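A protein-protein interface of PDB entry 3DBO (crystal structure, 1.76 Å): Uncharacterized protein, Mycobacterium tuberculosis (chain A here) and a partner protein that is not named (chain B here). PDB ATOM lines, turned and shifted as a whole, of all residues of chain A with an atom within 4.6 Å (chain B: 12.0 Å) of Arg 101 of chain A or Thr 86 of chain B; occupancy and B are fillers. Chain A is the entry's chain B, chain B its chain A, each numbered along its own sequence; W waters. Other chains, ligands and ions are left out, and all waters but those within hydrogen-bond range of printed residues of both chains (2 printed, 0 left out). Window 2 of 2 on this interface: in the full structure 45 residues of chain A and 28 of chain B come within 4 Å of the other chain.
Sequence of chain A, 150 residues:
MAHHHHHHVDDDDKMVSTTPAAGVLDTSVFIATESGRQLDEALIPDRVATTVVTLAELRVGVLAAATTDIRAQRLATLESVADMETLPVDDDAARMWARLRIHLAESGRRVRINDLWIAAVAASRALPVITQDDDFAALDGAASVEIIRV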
ATOM      1  N   TRP A  97     -21.967 -19.845   1.053  1.00  0.00           N
ATOM      2  CA  TRP A  97     -21.105 -18.997   1.871  1.00  0.00           C
ATOM      3  C   TRP A  97     -20.528 -17.867   1.015  1.00  0.00           C
ATOM      4  O   TRP A  97     -20.525 -16.724   1.450  1.00  0.00           O
ATOM      5  CB  TRP A  97     -19.961 -19.807   2.482  1.00  0.00           C
ATOM      6  CG  TRP A  97     -19.100 -19.096   3.505  1.00  0.00           C
ATOM      7  CD1 TRP A  97     -19.256 -19.112   4.859  1.00  0.00           C
ATOM      8  CD2 TRP A  97     -17.942 -18.303   3.239  1.00  0.00           C
ATOM      9  NE1 TRP A  97     -18.253 -18.380   5.459  1.00  0.00           N
ATOM     10  CE2 TRP A  97     -17.440 -17.865   4.480  1.00  0.00           C
ATOM     11  CE3 TRP A  97     -17.277 -17.919   2.059  1.00  0.00           C
ATOM     12  CZ2 TRP A  97     -16.288 -17.067   4.588  1.00  0.00           C
ATOM     13  CZ3 TRP A  97     -16.133 -17.112   2.174  1.00  0.00           C
ATOM     14  CH2 TRP A  97     -15.655 -16.706   3.421  1.00  0.00           C
ATOM     15  N   ALA A  98     -20.072 -18.191  -0.191  1.00  0.00           N
ATOM     16  CA  ALA A  98     -19.501 -17.174  -1.078  1.00  0.00           C
ATOM     17  C   ALA A  98     -20.526 -16.078  -1.432  1.00  0.00           C
ATOM     18  O   ALA A  98     -20.191 -14.896  -1.401  1.00  0.00           O
ATOM     19  CB  ALA A  98     -18.935 -17.838  -2.371  1.00  0.00           C
ATOM     20  N   ARG A  99     -21.740 -16.475  -1.806  1.00  0.00           N
ATOM     21  CA  ARG A  99     -22.813 -15.529  -2.142  1.00  0.00           C
ATOM     22  C   ARG A  99     -23.117 -14.617  -0.950  1.00  0.00           C
ATOM     23  O   ARG A  99     -23.168 -13.390  -1.094  1.00  0.00           O
ATOM     24  CB  ARG A  99     -24.095 -16.279  -2.558  1.00  0.00           C
ATOM     25  CG  ARG A  99     -25.217 -15.356  -3.035  1.00  0.00           C
ATOM     26  CD  ARG A  99     -26.352 -16.094  -3.764  1.00  0.00           C
ATOM     27  NE  ARG A  99     -27.251 -15.116  -4.385  1.00  0.00           N
ATOM     28  CZ  ARG A  99     -28.025 -15.340  -5.447  1.00  0.00           C
ATOM     29  NH1 ARG A  99     -28.024 -16.524  -6.049  1.00  0.00           N
ATOM     30  NH2 ARG A  99     -28.796 -14.357  -5.922  1.00  0.00           N
ATOM     31  N   LEU A 100     -23.314 -15.228   0.214  1.00  0.00           N
ATOM     32  CA  LEU A 100     -23.626 -14.459   1.434  1.00  0.00           C
ATOM     33  C   LEU A 100     -22.470 -13.545   1.843  1.00  0.00           C
ATOM     34  O   LEU A 100     -22.682 -12.393   2.241  1.00  0.00           O
ATOM     35  CB  LEU A 100     -24.060 -15.389   2.582  1.00  0.00           C
ATOM     36  CG  LEU A 100     -25.301 -16.259   2.332  1.00  0.00           C
ATOM     37  CD1 LEU A 100     -25.557 -17.174   3.529  1.00  0.00           C
ATOM     38  CD2 LEU A 100     -26.535 -15.406   1.999  1.00  0.00           C
ATOM     39  N   ARG A 101     -21.242 -14.044   1.725  1.00  0.00           N
ATOM     40  CA  ARG A 101     -20.052 -13.250   2.019  1.00  0.00           C
ATOM     41  C   ARG A 101     -19.924 -12.004   1.138  1.00  0.00           C
ATOM     42  O   ARG A 101     -19.599 -10.919   1.638  1.00  0.00           O
ATOM     43  CB  ARG A 101     -18.762 -14.099   1.925  1.00  0.00           C
ATOM     44  CG  ARG A 101     -17.491 -13.364   2.365  1.00  0.00           C
ATOM     45  CD  ARG A 101     -17.539 -12.997   3.830  1.00  0.00           C
ATOM     46  NE  ARG A 101     -16.579 -11.952   4.205  1.00  0.00           N
ATOM     47  CZ  ARG A 101     -16.834 -10.642   4.192  1.00  0.00           C
ATOM     48  NH1 ARG A 101     -17.999 -10.184   3.794  1.00  0.00           N
ATOM     49  NH2 ARG A 101     -15.901  -9.781   4.595  1.00  0.00           N
ATOM     50  N   ILE A 102     -20.171 -12.147  -0.157  1.00  0.00           N
ATOM     51  CA  ILE A 102     -20.081 -10.959  -1.028  1.00  0.00           C
ATOM     52  C   ILE A 102     -21.245  -9.977  -0.737  1.00  0.00           C
ATOM     53  O   ILE A 102     -21.030  -8.764  -0.691  1.00  0.00           O
ATOM     54  CB  ILE A 102     -20.037 -11.358  -2.533  1.00  0.00           C
ATOM     55  CG1 ILE A 102     -18.630 -11.791  -2.894  1.00  0.00           C
ATOM     56  CG2 ILE A 102     -20.295 -10.160  -3.458  1.00  0.00           C
ATOM     57  CD1 ILE A 102     -17.700 -10.628  -3.010  1.00  0.00           C
ATOM     58  N   HIS A 103     -22.433 -10.518  -0.476  1.00  0.00           N
ATOM     59  CA  HIS A 103     -23.580  -9.708  -0.057  1.00  0.00           C
ATOM     60  C   HIS A 103     -23.180  -8.793   1.115  1.00  0.00           C
ATOM     61  O   HIS A 103     -23.367  -7.564   1.051  1.00  0.00           O
ATOM     62  CB  HIS A 103     -24.763 -10.619   0.296  1.00  0.00           C
ATOM     63  CG  HIS A 103     -26.009  -9.880   0.679  1.00  0.00           C
ATOM     64  ND1 HIS A 103     -26.760  -9.169  -0.232  1.00  0.00           N
ATOM     65  CD2 HIS A 103     -26.639  -9.753   1.872  1.00  0.00           C
ATOM     66  CE1 HIS A 103     -27.800  -8.632   0.387  1.00  0.00           C
ATOM     67  NE2 HIS A 103     -27.744  -8.962   1.665  1.00  0.00           N
ATOM     68  N   LEU A 104     -22.577  -9.375   2.152  1.00  0.00           N
ATOM     69  CA  LEU A 104     -22.086  -8.600   3.302  1.00  0.00           C
ATOM     70  C   LEU A 104     -20.987  -7.584   2.950  1.00  0.00           C
ATOM     71  O   LEU A 104     -21.015  -6.449   3.445  1.00  0.00           O
ATOM     72  CB  LEU A 104     -21.608  -9.529   4.418  1.00  0.00           C
ATOM     73  CG  LEU A 104     -22.699 -10.343   5.115  1.00  0.00           C
ATOM     74  CD1 LEU A 104     -22.047 -11.554   5.854  1.00  0.00           C
ATOM     75  CD2 LEU A 104     -23.517  -9.460   6.071  1.00  0.00           C
ATOM     76  N   ALA A 105     -20.042  -7.972   2.085  1.00  0.00           N
ATOM     77  CA  ALA A 105     -18.908  -7.090   1.742  1.00  0.00           C
ATOM     78  C   ALA A 105     -19.416  -5.830   1.059  1.00  0.00           C
ATOM     79  O   ALA A 105     -18.964  -4.711   1.357  1.00  0.00           O
ATOM     80  CB  ALA A 105     -17.932  -7.801   0.850  1.00  0.00           C
ATOM     81  N   ARG A 109     -21.526  -4.720   5.910  1.00  0.00           N
ATOM     82  CA  ARG A 109     -22.003  -5.314   7.160  1.00  0.00           C
ATOM     83  C   ARG A 109     -21.163  -6.545   7.545  1.00  0.00           C
ATOM     84  O   ARG A 109     -20.444  -7.092   6.706  1.00  0.00           O
ATOM     85  CB  ARG A 109     -23.478  -5.714   7.044  1.00  0.00           C
ATOM     86  CG  ARG A 109     -24.487  -4.556   7.128  1.00  0.00           C
ATOM     87  CD  ARG A 109     -25.924  -5.088   7.071  1.00  0.00           C
ATOM     88  NE  ARG A 109     -26.038  -6.173   6.102  1.00  0.00           N
ATOM     89  CZ  ARG A 109     -26.494  -6.039   4.862  1.00  0.00           C
ATOM     90  NH1 ARG A 109     -26.919  -4.860   4.423  1.00  0.00           N
ATOM     91  NH2 ARG A 109     -26.534  -7.091   4.067  1.00  0.00           N
ATOM     92  N   ARG A 110     -21.248  -6.965   8.809  1.00  0.00           N
ATOM     93  CA  ARG A 110     -20.425  -8.072   9.303  1.00  0.00           C
ATOM     94  C   ARG A 110     -21.214  -9.167  10.024  1.00  0.00           C
ATOM     95  O   ARG A 110     -22.231  -8.892  10.664  1.00  0.00           O
ATOM     96  CB  ARG A 110     -19.306  -7.548  10.214  1.00  0.00           C
ATOM     97  CG  ARG A 110     -18.316  -6.608   9.525  1.00  0.00           C
ATOM     98  CD  ARG A 110     -17.348  -5.958  10.511  1.00  0.00           C
ATOM     99  NE  ARG A 110     -18.034  -5.112  11.484  1.00  0.00           N
ATOM    100  CZ  ARG A 110     -18.282  -5.470  12.740  1.00  0.00           C
ATOM    101  NH1 ARG A 110     -17.897  -6.661  13.177  1.00  0.00           N
ATOM    102  NH2 ARG A 110     -18.916  -4.637  13.557  1.00  0.00           N
ATOM    103  N   VAL A 111     -20.704 -10.400   9.911  1.00  0.00           N
ATOM    104  CA  VAL A 111     -21.185 -11.581  10.637  1.00  0.00           C
ATOM    105  C   VAL A 111     -19.898 -12.321  11.078  1.00  0.00           C
ATOM    106  O   VAL A 111     -18.956 -12.350  10.292  1.00  0.00           O
ATOM    107  CB  VAL A 111     -22.043 -12.475   9.663  1.00  0.00           C
ATOM    108  CG1 VAL A 111     -22.270 -13.858  10.195  1.00  0.00           C
ATOM    109  CG2 VAL A 111     -23.415 -11.795   9.307  1.00  0.00           C
ATOM    110  N   ILE A 113     -17.331 -15.158  11.242  1.00  0.00           N
ATOM    111  CA  ILE A 113     -17.156 -16.086  10.115  1.00  0.00           C
ATOM    112  C   ILE A 113     -17.798 -17.463  10.375  1.00  0.00           C
ATOM    113  O   ILE A 113     -18.380 -18.055   9.465  1.00  0.00           O
ATOM    114  CB  ILE A 113     -15.680 -16.195   9.625  1.00  0.00           C
ATOM    115  CG1 ILE A 113     -15.626 -16.855   8.243  1.00  0.00           C
ATOM    116  CG2 ILE A 113     -14.828 -16.971  10.609  1.00  0.00           C
ATOM    117  CD1 ILE A 113     -14.299 -16.673   7.506  1.00  0.00           C
ATOM    118  N   LEU A 116     -21.365 -17.245   9.752  1.00  0.00           N
ATOM    119  CA  LEU A 116     -21.650 -17.245   8.301  1.00  0.00           C
ATOM    120  C   LEU A 116     -21.669 -18.659   7.722  1.00  0.00           C
ATOM    121  O   LEU A 116     -22.527 -18.980   6.888  1.00  0.00           O
ATOM    122  CB  LEU A 116     -20.669 -16.351   7.530  1.00  0.00           C
ATOM    123  CG  LEU A 116     -21.054 -16.060   6.066  1.00  0.00           C
ATOM    124  CD1 LEU A 116     -22.453 -15.365   5.936  1.00  0.00           C
ATOM    125  CD2 LEU A 116     -19.930 -15.196   5.450  1.00  0.00           C
ATOM    126  N   ALA B  79     -16.084 -15.860  22.129  1.00  0.00           N
ATOM    127  CA  ALA B  79     -15.659 -14.560  21.573  1.00  0.00           C
ATOM    128  C   ALA B  79     -14.133 -14.527  21.354  1.00  0.00           C
ATOM    129  O   ALA B  79     -13.640 -14.038  20.331  1.00  0.00           O
ATOM    130  CB  ALA B  79     -16.111 -13.416  22.470  1.00  0.00           C
ATOM    131  N   ALA B  82     -13.442 -17.929  18.643  1.00  0.00           N
ATOM    132  CA  ALA B  82     -14.163 -18.011  17.368  1.00  0.00           C
ATOM    133  C   ALA B  82     -14.996 -16.751  17.101  1.00  0.00           C
ATOM    134  O   ALA B  82     -16.045 -16.810  16.426  1.00  0.00           O
ATOM    135  CB  ALA B  82     -15.057 -19.261  17.353  1.00  0.00           C
ATOM    136  N   GLY B  83     -14.532 -15.619  17.641  1.00  0.00           N
ATOM    137  CA  GLY B  83     -15.253 -14.344  17.537  1.00  0.00           C
ATOM    138  C   GLY B  83     -14.839 -13.523  16.327  1.00  0.00           C
ATOM    139  O   GLY B  83     -15.327 -12.409  16.117  1.00  0.00           O
ATOM    140  N   ASP B  84     -13.944 -14.085  15.526  1.00  0.00           N
ATOM    141  CA  ASP B  84     -13.483 -13.459  14.285  1.00  0.00           C
ATOM    142  C   ASP B  84     -14.627 -13.235  13.299  1.00  0.00           C
ATOM    143  O   ASP B  84     -15.366 -14.162  12.993  1.00  0.00           O
ATOM    144  CB  ASP B  84     -12.386 -14.311  13.647  1.00  0.00           C
ATOM    145  CG  ASP B  84     -12.810 -15.765  13.426  1.00  0.00           C
ATOM    146  OD1 ASP B  84     -13.459 -16.356  14.320  1.00  0.00           O
ATOM    147  OD2 ASP B  84     -12.485 -16.320  12.356  1.00  0.00           O
ATOM    148  N   THR B  85     -14.753 -11.999  12.814  1.00  0.00           N
ATOM    149  CA  THR B  85     -15.848 -11.605  11.914  1.00  0.00           C
ATOM    150  C   THR B  85     -15.401 -11.587  10.445  1.00  0.00           C
ATOM    151  O   THR B  85     -14.232 -11.844  10.126  1.00  0.00           O
ATOM    152  CB  THR B  85     -16.468 -10.221  12.295  1.00  0.00           C
ATOM    153  OG1 THR B  85     -15.600  -9.161  11.864  1.00  0.00           O
ATOM    154  CG2 THR B  85     -16.705 -10.105  13.807  1.00  0.00           C
ATOM    155  N   THR B  86     -16.343 -11.292   9.554  1.00  0.00           N
ATOM    156  CA  THR B  86     -16.049 -11.246   8.130  1.00  0.00           C
ATOM    157  C   THR B  86     -15.144 -10.055   7.824  1.00  0.00           C
ATOM    158  O   THR B  86     -14.332 -10.107   6.897  1.00  0.00           O
ATOM    159  CB  THR B  86     -17.344 -11.216   7.274  1.00  0.00           C
ATOM    160  OG1 THR B  86     -18.263 -10.245   7.790  1.00  0.00           O
ATOM    161  CG2 THR B  86     -18.000 -12.588   7.258  1.00  0.00           C
HETATM  162  O   HOH W   1     -18.198  -8.038   5.649  1.00  0.00           O
HETATM  163  O   HOH W   2     -16.024 -16.796  13.745  1.00  0.00           O
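The backbone carbonyl oxygen (O) of Asp 84 of chain B lies within hydrogen-bond range of the backbone NH (N) of Ile 113 of chain A (2.8 Å). The backbone carbonyl oxygen of Val 111 of chain A sits at hydrogen-bond distance from the backbone NH of Thr 86 of chain B (2.9 Å). O of Thr 86 of chain B lies within hydrogen-bond range of NH2 of Arg 101 of chain A (2.8 Å).
No residue of chain B comes within 4 Å of Trp 97 of chain A. Arg 101 of chain A touches just one residue of chain B: Thr 86. No residue of chain B comes within 4 Å of Leu 104 of chain A. No residue of chain B comes within 4 Å of Ala 105 of chain A. Printed residues of chain B within 4 Å of Arg 110 of chain A: Thr 85 and Thr 86. Leu 116 of chain A touches just one residue of chain B: Thr 86. Printed residues of chain A within 4 Å of Asp 84 of chain B: Ile 113 (2.8 Å). The nearest printed residue of chain A that does not touch Thr 86 of chain B is Ile 113 of chain A (4.3 Å). The nearest printed residue of chain A that does not touch Asp 84 of chain B is Val 111 of chain A (4.8 Å).
A ring nitrogen (NE2) of His 103 of chain A lies within hydrogen-bond range of the guanidinium group (NH2) of Arg 109 of chain A, 3.3 Å away. The backbone NH (N) of Arg 109 of chain A lies within hydrogen-bond range of the backbone carbonyl oxygen (O) of Leu 104 of chain A (3.1 Å).
Among the printed residues, merely in contact across the chains: Arg 109 of chain A with Thr 86 of chain B, Arg 110 of chain A with Thr 85 of chain B, Arg 110 of chain A with Thr 86 of chain B, Val 111 of chain A with Thr 85 of chain B, Ile 113 of chain A with Thr 85 of chain B and Leu 116 of chain A with Thr 86 of chain B.
Water W1 lies within hydrogen-bond range of the backbone carbonyl oxygen (O) of Arg 109 of chain A (2.7 Å), the guanidinium group (NH1) of Arg 101 of chain A (2.8 Å) and the side-chain hydroxyl (OG1) of Thr 86 of chain B (3.1 Å). Water W2 lies within hydrogen-bond range of the side-chain carboxylate of Asp 84 of chain B (2.7 Å), the backbone carbonyl oxygen of Ala 82 of chain B (2.7 Å) and the backbone NH of Ile 113 of chain A (3.3 Å).
Hydrophobic or aromatic side chains of chain A within 4 Å of the printed part of chain B: Ile 113 and Leu 116. Among the printed residues, no Asp or Glu carboxylate lies within 4 Å of a Lys or Arg side-chain nitrogen of the other chain.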
